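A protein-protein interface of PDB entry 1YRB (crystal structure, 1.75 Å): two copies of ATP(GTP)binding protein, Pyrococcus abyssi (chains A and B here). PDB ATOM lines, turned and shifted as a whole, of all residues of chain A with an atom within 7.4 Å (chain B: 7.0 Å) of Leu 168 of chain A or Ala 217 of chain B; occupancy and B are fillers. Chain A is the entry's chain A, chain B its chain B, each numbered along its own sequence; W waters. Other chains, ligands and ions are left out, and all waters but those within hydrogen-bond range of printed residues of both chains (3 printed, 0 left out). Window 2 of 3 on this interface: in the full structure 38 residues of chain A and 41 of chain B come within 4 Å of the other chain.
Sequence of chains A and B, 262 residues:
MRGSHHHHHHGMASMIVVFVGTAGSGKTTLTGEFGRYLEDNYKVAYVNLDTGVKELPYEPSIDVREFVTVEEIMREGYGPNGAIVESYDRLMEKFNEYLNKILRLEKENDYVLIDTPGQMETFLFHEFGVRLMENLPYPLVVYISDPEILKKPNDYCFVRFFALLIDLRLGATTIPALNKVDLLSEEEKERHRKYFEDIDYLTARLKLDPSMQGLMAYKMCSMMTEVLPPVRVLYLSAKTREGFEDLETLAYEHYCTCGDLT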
ATOM      1  N   VAL A 130      11.955  35.951   6.165  1.00  0.00           N
ATOM      2  CA  VAL A 130      11.847  35.251   4.882  1.00  0.00           C
ATOM      3  C   VAL A 130      12.373  36.096   3.693  1.00  0.00           C
ATOM      4  O   VAL A 130      12.998  35.574   2.764  1.00  0.00           O
ATOM      5  CB  VAL A 130      10.381  34.836   4.634  1.00  0.00           C
ATOM      6  CG1 VAL A 130      10.265  33.910   3.437  1.00  0.00           C
ATOM      7  CG2 VAL A 130       9.814  34.183   5.900  1.00  0.00           C
ATOM      8  N   PHE A 162      10.221  19.255  10.800  1.00  0.00           N
ATOM      9  CA  PHE A 162      10.293  20.691  11.045  1.00  0.00           C
ATOM     10  C   PHE A 162      11.480  21.310  10.308  1.00  0.00           C
ATOM     11  O   PHE A 162      11.387  22.407   9.747  1.00  0.00           O
ATOM     12  CB  PHE A 162      10.320  21.017  12.537  1.00  0.00           C
ATOM     13  CG  PHE A 162       9.895  22.428  12.843  1.00  0.00           C
ATOM     14  CD1 PHE A 162       8.552  22.748  12.923  1.00  0.00           C
ATOM     15  CD2 PHE A 162      10.829  23.432  13.005  1.00  0.00           C
ATOM     16  CE1 PHE A 162       8.151  24.048  13.182  1.00  0.00           C
ATOM     17  CE2 PHE A 162      10.441  24.730  13.259  1.00  0.00           C
ATOM     18  CZ  PHE A 162       9.107  25.041  13.340  1.00  0.00           C
ATOM     19  N   ALA A 163      12.599  20.597  10.282  1.00  0.00           N
ATOM     20  CA  ALA A 163      13.773  21.066   9.556  1.00  0.00           C
ATOM     21  C   ALA A 163      13.492  21.145   8.046  1.00  0.00           C
ATOM     22  O   ALA A 163      13.922  22.079   7.362  1.00  0.00           O
ATOM     23  CB  ALA A 163      14.980  20.168   9.866  1.00  0.00           C
ATOM     24  N   LEU A 164      12.755  20.166   7.533  1.00  0.00           N
ATOM     25  CA  LEU A 164      12.353  20.159   6.134  1.00  0.00           C
ATOM     26  C   LEU A 164      11.474  21.374   5.805  1.00  0.00           C
ATOM     27  O   LEU A 164      11.640  22.013   4.760  1.00  0.00           O
ATOM     28  CB  LEU A 164      11.598  18.858   5.817  1.00  0.00           C
ATOM     29  CG  LEU A 164      12.381  17.628   5.339  1.00  0.00           C
ATOM     30  CD1 LEU A 164      13.761  17.513   5.976  1.00  0.00           C
ATOM     31  CD2 LEU A 164      11.566  16.366   5.582  1.00  0.00           C
ATOM     32  N   LEU A 165      10.572  21.699   6.725  1.00  0.00           N
ATOM     33  CA  LEU A 165       9.660  22.819   6.577  1.00  0.00           C
ATOM     34  C   LEU A 165      10.456  24.120   6.549  1.00  0.00           C
ATOM     35  O   LEU A 165      10.170  25.019   5.772  1.00  0.00           O
ATOM     36  CB  LEU A 165       8.683  22.842   7.739  1.00  0.00           C
ATOM     37  CG  LEU A 165       7.174  22.803   7.502  1.00  0.00           C
ATOM     38  CD1 LEU A 165       6.511  23.748   8.484  1.00  0.00           C
ATOM     39  CD2 LEU A 165       6.787  23.138   6.074  1.00  0.00           C
ATOM     40  N   ILE A 166      11.460  24.223   7.411  1.00  0.00           N
ATOM     41  CA  ILE A 166      12.311  25.406   7.432  1.00  0.00           C
ATOM     42  C   ILE A 166      13.042  25.567   6.115  1.00  0.00           C
ATOM     43  O   ILE A 166      13.145  26.676   5.572  1.00  0.00           O
ATOM     44  CB  ILE A 166      13.342  25.316   8.564  1.00  0.00           C
ATOM     45  CG1 ILE A 166      12.646  25.564   9.901  1.00  0.00           C
ATOM     46  CG2 ILE A 166      14.479  26.311   8.315  1.00  0.00           C
ATOM     47  CD1 ILE A 166      13.426  25.054  11.104  1.00  0.00           C
ATOM     48  N   ASP A 167      13.554  24.458   5.593  1.00  0.00           N
ATOM     49  CA  ASP A 167      14.277  24.453   4.324  1.00  0.00           C
ATOM     50  C   ASP A 167      13.359  24.960   3.212  1.00  0.00           C
ATOM     51  O   ASP A 167      13.762  25.787   2.388  1.00  0.00           O
ATOM     52  CB  ASP A 167      14.771  23.033   4.031  1.00  0.00           C
ATOM     53  CG  ASP A 167      15.769  22.973   2.888  1.00  0.00           C
ATOM     54  OD1 ASP A 167      15.572  23.677   1.878  1.00  0.00           O
ATOM     55  OD2 ASP A 167      16.750  22.205   3.001  1.00  0.00           O
ATOM     56  N   LEU A 168      12.120  24.473   3.208  1.00  0.00           N
ATOM     57  CA  LEU A 168      11.115  24.922   2.242  1.00  0.00           C
ATOM     58  C   LEU A 168      10.837  26.406   2.399  1.00  0.00           C
ATOM     59  O   LEU A 168      10.882  27.168   1.433  1.00  0.00           O
ATOM     60  CB  LEU A 168       9.806  24.162   2.434  1.00  0.00           C
ATOM     61  CG  LEU A 168       8.678  24.632   1.513  1.00  0.00           C
ATOM     62  CD1 LEU A 168       9.006  24.251   0.059  1.00  0.00           C
ATOM     63  CD2 LEU A 168       7.336  24.060   1.947  1.00  0.00           C
ATOM     64  N   ARG A 169      10.547  26.806   3.628  1.00  0.00           N
ATOM     65  CA  ARG A 169      10.184  28.179   3.936  1.00  0.00           C
ATOM     66  C   ARG A 169      11.302  29.168   3.592  1.00  0.00           C
ATOM     67  O   ARG A 169      11.061  30.192   2.932  1.00  0.00           O
ATOM     68  CB  ARG A 169       9.815  28.278   5.422  1.00  0.00           C
ATOM     69  CG  ARG A 169       9.358  29.640   5.886  1.00  0.00           C
ATOM     70  CD  ARG A 169       8.140  30.100   5.116  1.00  0.00           C
ATOM     71  NE  ARG A 169       7.623  31.327   5.695  1.00  0.00           N
ATOM     72  CZ  ARG A 169       6.807  32.173   5.076  1.00  0.00           C
ATOM     73  NH1 ARG A 169       6.425  31.945   3.824  1.00  0.00           N
ATOM     74  NH2 ARG A 169       6.400  33.260   5.702  1.00  0.00           N
ATOM     75  N   LEU A 170      12.525  28.855   4.008  1.00  0.00           N
ATOM     76  CA  LEU A 170      13.655  29.773   3.830  1.00  0.00           C
ATOM     77  C   LEU A 170      14.437  29.575   2.536  1.00  0.00           C
ATOM     78  O   LEU A 170      15.225  30.433   2.151  1.00  0.00           O
ATOM     79  CB  LEU A 170      14.599  29.698   5.029  1.00  0.00           C
ATOM     80  CG  LEU A 170      13.900  29.995   6.357  1.00  0.00           C
ATOM     81  CD1 LEU A 170      14.900  29.931   7.489  1.00  0.00           C
ATOM     82  CD2 LEU A 170      13.149  31.344   6.344  1.00  0.00           C
ATOM     83  N   GLY A 171      14.218  28.445   1.872  1.00  0.00           N
ATOM     84  CA  GLY A 171      14.881  28.159   0.615  1.00  0.00           C
ATOM     85  C   GLY A 171      16.369  28.000   0.785  1.00  0.00           C
ATOM     86  O   GLY A 171      17.145  28.315  -0.118  1.00  0.00           O
ATOM     87  N   ALA A 172      16.764  27.474   1.939  1.00  0.00           N
ATOM     88  CA  ALA A 172      18.171  27.288   2.255  1.00  0.00           C
ATOM     89  C   ALA A 172      18.425  25.887   2.784  1.00  0.00           C
ATOM     90  O   ALA A 172      17.563  25.308   3.448  1.00  0.00           O
ATOM     91  CB  ALA A 172      18.616  28.327   3.294  1.00  0.00           C
ATOM     92  N   THR A 174      19.185  23.321   5.228  1.00  0.00           N
ATOM     93  CA  THR A 174      18.983  23.344   6.667  1.00  0.00           C
ATOM     94  C   THR A 174      19.532  22.069   7.287  1.00  0.00           C
ATOM     95  O   THR A 174      19.162  20.961   6.885  1.00  0.00           O
ATOM     96  CB  THR A 174      17.502  23.537   7.016  1.00  0.00           C
ATOM     97  OG1 THR A 174      17.070  24.783   6.472  1.00  0.00           O
ATOM     98  CG2 THR A 174      17.280  23.540   8.506  1.00  0.00           C
ATOM     99  N   LYS B 152       2.332  33.141  -2.554  1.00  0.00           N
ATOM    100  CA  LYS B 152       2.603  32.239  -3.671  1.00  0.00           C
ATOM    101  C   LYS B 152       2.243  30.801  -3.290  1.00  0.00           C
ATOM    102  O   LYS B 152       2.130  30.479  -2.104  1.00  0.00           O
ATOM    103  CB  LYS B 152       4.085  32.323  -4.041  1.00  0.00           C
ATOM    104  CG  LYS B 152       5.022  31.786  -2.969  1.00  0.00           C
ATOM    105  CD  LYS B 152       6.465  32.175  -3.261  1.00  0.00           C
ATOM    106  CE  LYS B 152       7.448  31.393  -2.406  1.00  0.00           C
ATOM    107  NZ  LYS B 152       7.421  31.781  -0.970  1.00  0.00           N
ATOM    108  N   PRO B 153       2.054  29.924  -4.292  1.00  0.00           N
ATOM    109  CA  PRO B 153       1.671  28.537  -4.008  1.00  0.00           C
ATOM    110  C   PRO B 153       2.464  27.849  -2.887  1.00  0.00           C
ATOM    111  O   PRO B 153       1.875  27.132  -2.076  1.00  0.00           O
ATOM    112  CB  PRO B 153       1.925  27.836  -5.347  1.00  0.00           C
ATOM    113  CG  PRO B 153       1.603  28.889  -6.349  1.00  0.00           C
ATOM    114  CD  PRO B 153       2.137  30.176  -5.749  1.00  0.00           C
ATOM    115  N   ASN B 154       3.781  28.034  -2.858  1.00  0.00           N
ATOM    116  CA  ASN B 154       4.610  27.365  -1.855  1.00  0.00           C
ATOM    117  C   ASN B 154       4.175  27.764  -0.430  1.00  0.00           C
ATOM    118  O   ASN B 154       4.307  26.982   0.515  1.00  0.00           O
ATOM    119  CB  ASN B 154       6.091  27.720  -2.055  1.00  0.00           C
ATOM    120  CG  ASN B 154       6.718  27.009  -3.245  1.00  0.00           C
ATOM    121  OD1 ASN B 154       7.813  27.373  -3.699  1.00  0.00           O
ATOM    122  ND2 ASN B 154       6.040  25.993  -3.750  1.00  0.00           N
ATOM    123  N   ASP B 155       3.657  28.985  -0.280  1.00  0.00           N
ATOM    124  CA  ASP B 155       3.241  29.478   1.050  1.00  0.00           C
ATOM    125  C   ASP B 155       2.039  28.674   1.567  1.00  0.00           C
ATOM    126  O   ASP B 155       1.913  28.424   2.772  1.00  0.00           O
ATOM    127  CB  ASP B 155       2.878  30.971   1.000  1.00  0.00           C
ATOM    128  CG  ASP B 155       3.998  31.840   0.444  1.00  0.00           C
ATOM    129  OD1 ASP B 155       5.189  31.502   0.623  1.00  0.00           O
ATOM    130  OD2 ASP B 155       3.686  32.872  -0.192  1.00  0.00           O
ATOM    131  N   CYS B 157       1.480  25.596   0.855  1.00  0.00           N
ATOM    132  CA  CYS B 157       2.045  24.305   1.236  1.00  0.00           C
ATOM    133  C   CYS B 157       2.604  24.426   2.655  1.00  0.00           C
ATOM    134  O   CYS B 157       2.288  23.625   3.524  1.00  0.00           O
ATOM    135  CB  CYS B 157       3.145  23.885   0.250  1.00  0.00           C
ATOM    136  SG  CYS B 157       4.021  22.368   0.710  1.00  0.00           S
ATOM    137  N   PHE B 158       3.397  25.469   2.877  1.00  0.00           N
ATOM    138  CA  PHE B 158       4.022  25.726   4.179  1.00  0.00           C
ATOM    139  C   PHE B 158       2.980  25.729   5.288  1.00  0.00           C
ATOM    140  O   PHE B 158       3.110  25.041   6.291  1.00  0.00           O
ATOM    141  CB  PHE B 158       4.769  27.064   4.129  1.00  0.00           C
ATOM    142  CG  PHE B 158       5.318  27.528   5.464  1.00  0.00           C
ATOM    143  CD1 PHE B 158       6.254  26.771   6.140  1.00  0.00           C
ATOM    144  CD2 PHE B 158       4.919  28.741   6.017  1.00  0.00           C
ATOM    145  CE1 PHE B 158       6.773  27.202   7.366  1.00  0.00           C
ATOM    146  CE2 PHE B 158       5.433  29.170   7.251  1.00  0.00           C
ATOM    147  CZ  PHE B 158       6.360  28.389   7.909  1.00  0.00           C
ATOM    148  N   VAL B 159       1.919  26.497   5.104  1.00  0.00           N
ATOM    149  CA  VAL B 159       0.940  26.614   6.162  1.00  0.00           C
ATOM    150  C   VAL B 159       0.155  25.313   6.391  1.00  0.00           C
ATOM    151  O   VAL B 159      -0.128  24.924   7.528  1.00  0.00           O
ATOM    152  CB  VAL B 159       0.018  27.821   5.882  1.00  0.00           C
ATOM    153  CG1 VAL B 159      -1.179  27.769   6.751  1.00  0.00           C
ATOM    154  CG2 VAL B 159       0.822  29.101   6.118  1.00  0.00           C
ATOM    155  N   PHE B 161       1.249  22.260   5.692  1.00  0.00           N
ATOM    156  CA  PHE B 161       2.173  21.306   6.295  1.00  0.00           C
ATOM    157  C   PHE B 161       2.409  21.624   7.782  1.00  0.00           C
ATOM    158  O   PHE B 161       2.489  20.721   8.620  1.00  0.00           O
ATOM    159  CB  PHE B 161       3.492  21.252   5.532  1.00  0.00           C
ATOM    160  CG  PHE B 161       4.165  19.920   5.635  1.00  0.00           C
ATOM    161  CD1 PHE B 161       5.055  19.661   6.667  1.00  0.00           C
ATOM    162  CD2 PHE B 161       3.881  18.922   4.720  1.00  0.00           C
ATOM    163  CE1 PHE B 161       5.671  18.416   6.785  1.00  0.00           C
ATOM    164  CE2 PHE B 161       4.490  17.656   4.827  1.00  0.00           C
ATOM    165  CZ  PHE B 161       5.387  17.416   5.859  1.00  0.00           C
ATOM    166  N   THR B 203      -1.399  20.586  -5.049  1.00  0.00           N
ATOM    167  CA  THR B 203      -0.365  19.639  -5.435  1.00  0.00           C
ATOM    168  C   THR B 203      -0.117  19.737  -6.933  1.00  0.00           C
ATOM    169  O   THR B 203       1.032  19.800  -7.388  1.00  0.00           O
ATOM    170  CB  THR B 203      -0.766  18.192  -5.092  1.00  0.00           C
ATOM    171  OG1 THR B 203      -1.071  18.090  -3.694  1.00  0.00           O
ATOM    172  CG2 THR B 203       0.376  17.238  -5.420  1.00  0.00           C
ATOM    173  N   LEU B 206       1.834  22.911  -7.764  1.00  0.00           N
ATOM    174  CA  LEU B 206       3.233  22.841  -7.338  1.00  0.00           C
ATOM    175  C   LEU B 206       4.040  21.982  -8.304  1.00  0.00           C
ATOM    176  O   LEU B 206       5.201  22.281  -8.581  1.00  0.00           O
ATOM    177  CB  LEU B 206       3.351  22.282  -5.929  1.00  0.00           C
ATOM    178  CG  LEU B 206       2.656  23.146  -4.869  1.00  0.00           C
ATOM    179  CD1 LEU B 206       2.670  22.438  -3.553  1.00  0.00           C
ATOM    180  CD2 LEU B 206       3.377  24.479  -4.756  1.00  0.00           C
ATOM    181  N   LYS B 207       3.418  20.916  -8.805  1.00  0.00           N
ATOM    182  CA  LYS B 207       4.081  20.018  -9.769  1.00  0.00           C
ATOM    183  C   LYS B 207       4.608  20.776 -10.995  1.00  0.00           C
ATOM    184  O   LYS B 207       5.616  20.384 -11.603  1.00  0.00           O
ATOM    185  CB  LYS B 207       3.128  18.880 -10.184  1.00  0.00           C
ATOM    186  CG  LYS B 207       3.818  17.592 -10.635  1.00  0.00           C
ATOM    187  CD  LYS B 207       2.789  16.545 -11.075  1.00  0.00           C
ATOM    188  CE  LYS B 207       3.433  15.361 -11.802  1.00  0.00           C
ATOM    189  NZ  LYS B 207       3.704  14.195 -10.914  1.00  0.00           N
ATOM    190  N   ASP B 209       6.047  23.665 -11.106  1.00  0.00           N
ATOM    191  CA  ASP B 209       7.205  24.507 -10.812  1.00  0.00           C
ATOM    192  C   ASP B 209       8.463  23.637 -10.860  1.00  0.00           C
ATOM    193  O   ASP B 209       8.636  22.766 -10.014  1.00  0.00           O
ATOM    194  CB  ASP B 209       7.016  25.126  -9.406  1.00  0.00           C
ATOM    195  CG  ASP B 209       8.169  26.044  -8.985  1.00  0.00           C
ATOM    196  OD1 ASP B 209       8.014  26.756  -7.957  1.00  0.00           O
ATOM    197  OD2 ASP B 209       9.223  26.053  -9.651  1.00  0.00           O
ATOM    198  N   SER B 211      11.580  24.317 -10.297  1.00  0.00           N
ATOM    199  CA  SER B 211      12.670  24.701  -9.388  1.00  0.00           C
ATOM    200  C   SER B 211      12.827  23.755  -8.194  1.00  0.00           C
ATOM    201  O   SER B 211      11.932  22.962  -7.894  1.00  0.00           O
ATOM    202  CB  SER B 211      12.444  26.122  -8.865  1.00  0.00           C
ATOM    203  OG  SER B 211      11.340  26.158  -7.968  1.00  0.00           O
ATOM    204  N   MET B 212      13.961  23.871  -7.502  1.00  0.00           N
ATOM    205  CA  MET B 212      14.264  23.043  -6.331  1.00  0.00           C
ATOM    206  C   MET B 212      13.202  23.207  -5.251  1.00  0.00           C
ATOM    207  O   MET B 212      12.737  22.230  -4.672  1.00  0.00           O
ATOM    208  CB  MET B 212      15.635  23.413  -5.749  1.00  0.00           C
ATOM    209  CG  MET B 212      16.776  23.431  -6.756  1.00  0.00           C
ATOM    210  SD  MET B 212      17.112  21.802  -7.447  1.00  0.00           S
ATOM    211  CE  MET B 212      18.550  22.134  -8.465  1.00  0.00           C
ATOM    212  N   GLN B 213      12.823  24.451  -4.988  1.00  0.00           N
ATOM    213  CA  GLN B 213      11.808  24.744  -3.994  1.00  0.00           C
ATOM    214  C   GLN B 213      10.452  24.163  -4.405  1.00  0.00           C
ATOM    215  O   GLN B 213       9.735  23.578  -3.584  1.00  0.00           O
ATOM    216  CB  GLN B 213      11.716  26.257  -3.774  1.00  0.00           C
ATOM    217  CG  GLN B 213      11.527  26.658  -2.334  1.00  0.00           C
ATOM    218  CD  GLN B 213      12.076  28.035  -2.050  1.00  0.00           C
ATOM    219  OE1 GLN B 213      11.760  28.640  -1.029  1.00  0.00           O
ATOM    220  NE2 GLN B 213      12.902  28.543  -2.957  1.00  0.00           N
ATOM    221  N   GLY B 214      10.099  24.319  -5.681  1.00  0.00           N
ATOM    222  CA  GLY B 214       8.828  23.797  -6.173  1.00  0.00           C
ATOM    223  C   GLY B 214       8.782  22.292  -6.041  1.00  0.00           C
ATOM    224  O   GLY B 214       7.772  21.724  -5.646  1.00  0.00           O
ATOM    225  N   LEU B 215       9.886  21.648  -6.394  1.00  0.00           N
ATOM    226  CA  LEU B 215      10.046  20.204  -6.242  1.00  0.00           C
ATOM    227  C   LEU B 215       9.821  19.797  -4.795  1.00  0.00           C
ATOM    228  O   LEU B 215       9.053  18.889  -4.504  1.00  0.00           O
ATOM    229  CB  LEU B 215      11.461  19.797  -6.651  1.00  0.00           C
ATOM    230  CG  LEU B 215      11.792  19.450  -8.102  1.00  0.00           C
ATOM    231  CD1 LEU B 215      10.795  19.996  -9.094  1.00  0.00           C
ATOM    232  CD2 LEU B 215      13.204  19.932  -8.426  1.00  0.00           C
ATOM    233  N   MET B 216      10.491  20.494  -3.886  1.00  0.00           N
ATOM    234  CA  MET B 216      10.355  20.193  -2.473  1.00  0.00           C
ATOM    235  C   MET B 216       8.904  20.353  -2.043  1.00  0.00           C
ATOM    236  O   MET B 216       8.344  19.459  -1.424  1.00  0.00           O
ATOM    237  CB  MET B 216      11.281  21.080  -1.635  1.00  0.00           C
ATOM    238  CG  MET B 216      11.258  20.741  -0.151  1.00  0.00           C
ATOM    239  SD  MET B 216      12.731  21.307   0.712  1.00  0.00           S
ATOM    240  CE  MET B 216      13.904  20.027   0.288  1.00  0.00           C
ATOM    241  N   ALA B 217       8.293  21.485  -2.387  1.00  0.00           N
ATOM    242  CA  ALA B 217       6.899  21.729  -2.022  1.00  0.00           C
ATOM    243  C   ALA B 217       6.014  20.631  -2.594  1.00  0.00           C
ATOM    244  O   ALA B 217       5.147  20.096  -1.917  1.00  0.00           O
ATOM    245  CB  ALA B 217       6.445  23.105  -2.514  1.00  0.00           C
ATOM    246  N   TYR B 218       6.262  20.271  -3.849  1.00  0.00           N
ATOM    247  CA  TYR B 218       5.480  19.227  -4.481  1.00  0.00           C
ATOM    248  C   TYR B 218       5.591  17.894  -3.720  1.00  0.00           C
ATOM    249  O   TYR B 218       4.582  17.249  -3.468  1.00  0.00           O
ATOM    250  CB  TYR B 218       5.863  19.081  -5.973  1.00  0.00           C
ATOM    251  CG  TYR B 218       5.331  17.806  -6.571  1.00  0.00           C
ATOM    252  CD1 TYR B 218       6.167  16.711  -6.763  1.00  0.00           C
ATOM    253  CD2 TYR B 218       3.985  17.680  -6.908  1.00  0.00           C
ATOM    254  CE1 TYR B 218       5.687  15.530  -7.282  1.00  0.00           C
ATOM    255  CE2 TYR B 218       3.488  16.495  -7.431  1.00  0.00           C
ATOM    256  CZ  TYR B 218       4.351  15.428  -7.617  1.00  0.00           C
ATOM    257  OH  TYR B 218       3.886  14.244  -8.133  1.00  0.00           O
ATOM    258  N   LYS B 219       6.804  17.497  -3.336  1.00  0.00           N
ATOM    259  CA  LYS B 219       6.996  16.268  -2.551  1.00  0.00           C
ATOM    260  C   LYS B 219       6.310  16.317  -1.185  1.00  0.00           C
ATOM    261  O   LYS B 219       5.700  15.335  -0.751  1.00  0.00           O
ATOM    262  CB  LYS B 219       8.486  15.955  -2.352  1.00  0.00           C
ATOM    263  CG  LYS B 219       9.228  15.544  -3.608  1.00  0.00           C
ATOM    264  CD  LYS B 219      10.638  15.116  -3.248  1.00  0.00           C
ATOM    265  CE  LYS B 219      11.590  15.243  -4.421  1.00  0.00           C
ATOM    266  NZ  LYS B 219      12.983  14.927  -3.989  1.00  0.00           N
ATOM    267  N   MET B 220       6.406  17.455  -0.504  1.00  0.00           N
ATOM    268  CA  MET B 220       5.805  17.559   0.819  1.00  0.00           C
ATOM    269  C   MET B 220       4.287  17.563   0.714  1.00  0.00           C
ATOM    270  O   MET B 220       3.602  16.892   1.483  1.00  0.00           O
ATOM    271  CB  MET B 220       6.317  18.802   1.565  1.00  0.00           C
ATOM    272  CG  MET B 220       7.795  18.718   1.854  1.00  0.00           C
ATOM    273  SD  MET B 220       8.484  20.197   2.610  1.00  0.00           S
ATOM    274  CE  MET B 220      10.220  19.771   2.630  1.00  0.00           C
ATOM    275  N   CYS B 221       3.765  18.303  -0.258  1.00  0.00           N
ATOM    276  CA  CYS B 221       2.323  18.382  -0.449  1.00  0.00           C
ATOM    277  C   CYS B 221       1.739  17.028  -0.846  1.00  0.00           C
ATOM    278  O   CYS B 221       0.669  16.635  -0.376  1.00  0.00           O
ATOM    279  CB  CYS B 221       1.975  19.433  -1.499  1.00  0.00           C
ATOM    280  SG  CYS B 221       0.344  20.134  -1.254  1.00  0.00           S
ATOM    281  N   SER B 222       2.449  16.313  -1.713  1.00  0.00           N
ATOM    282  CA  SER B 222       2.008  14.981  -2.116  1.00  0.00           C
ATOM    283  C   SER B 222       2.002  14.008  -0.932  1.00  0.00           C
ATOM    284  O   SER B 222       1.051  13.252  -0.752  1.00  0.00           O
ATOM    285  CB  SER B 222       2.842  14.454  -3.298  1.00  0.00           C
ATOM    286  OG  SER B 222       4.207  14.302  -2.949  1.00  0.00           O
ATOM    287  N   MET B 223       3.039  14.065  -0.097  1.00  0.00           N
ATOM    288  CA  MET B 223       3.109  13.238   1.105  1.00  0.00           C
ATOM    289  C   MET B 223       1.948  13.550   2.043  1.00  0.00           C
ATOM    290  O   MET B 223       1.379  12.665   2.687  1.00  0.00           O
ATOM    291  CB  MET B 223       4.416  13.484   1.855  1.00  0.00           C
ATOM    292  CG  MET B 223       4.683  12.470   2.940  1.00  0.00           C
ATOM    293  SD  MET B 223       5.538  13.178   4.350  1.00  0.00           S
ATOM    294  CE  MET B 223       4.201  14.073   5.131  1.00  0.00           C
HETATM  295  O   HOH W   1      15.366  22.564  -1.286  1.00  0.00           O
HETATM  296  O   HOH W   2      13.815  24.333  -0.511  1.00  0.00           O
HETATM  297  O   HOH W   3       6.743  29.623   1.982  1.00  0.00           O
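Of the 13 printed residues of chain A, 6 touch a printed residue of chain B.
Printed residues of chain B within 4 Å of Leu 168 of chain A: Cys 157, Gln 213 and Ala 217. Printed residues of chain B within 4 Å of Asp 167 of chain A: Met 216. Of the printed residues of chain A, Met 216 of chain B touches Asp 167 (3.9 Å). The nearest printed residue of chain A that does not touch Ala 217 of chain B is Leu 164 of chain A (7.9 Å). The nearest printed residue of chain B that does not touch Leu 165 of chain A is Met 220 of chain B (4.5 Å).
Among the printed residues, merely in contact across the chains: Leu 164 of chain A with Met 220 of chain B, Arg 169 of chain A with Phe 158 of chain B, Gly 171 of chain A with Gln 213 of chain B, Leu 165 of chain A with Phe 158 of chain B, Leu 168 of chain A with Ala 217 of chain B, Leu 165 of chain A with Phe 161 of chain B, Asp 167 of chain A with Met 216 of chain B and Leu 168 of chain A with Cys 157 of chain B.
No position is printed for both chains. Of the 10 pairs that touch across the chains among the printed residues, none has its exchanged pair printed and touching as well.
O of Leu 168 of chain A lies close to OE1 of Gln 213 of chain B (3.0 Å). OD1 of Asp 155 of chain B lies within salt-bridge range of NH1 of Arg 169 of chain A (3.5 Å).
Water W3 lies within hydrogen-bond range of OD1 of Asp 155 of chain B (2.8 Å) and NH1 of Arg 169 of chain A (3.0 Å). Water W2 lies within hydrogen-bond range of OD1 of Asp 167 of chain A (3.0 Å) and SD of Met 216 of chain B (3.4 Å). Water W1 lies within hydrogen-bond range of the side-chain carboxylate of Asp 167 of chain A and the side-chain sulfur of Met 216 of chain B.
N of Thr 174 of chain A is in hydrogen-bond range of OD2 of Asp 167 of chain A, 3.5 Å away. The side-chain sulfur of Cys 157 of chain B sits at hydrogen-bond distance from the backbone carbonyl oxygen of Ala 217 of chain B (3.7 Å). NZ of Lys 152 of chain B lies within salt-bridge range of OD1 of Asp 155 of chain B, 2.8 Å away. The backbone carbonyl oxygen (O) of Asp 167 of chain A is in hydrogen-bond range of the backbone NH (N) of Ala 172 of chain A (3.5 Å).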
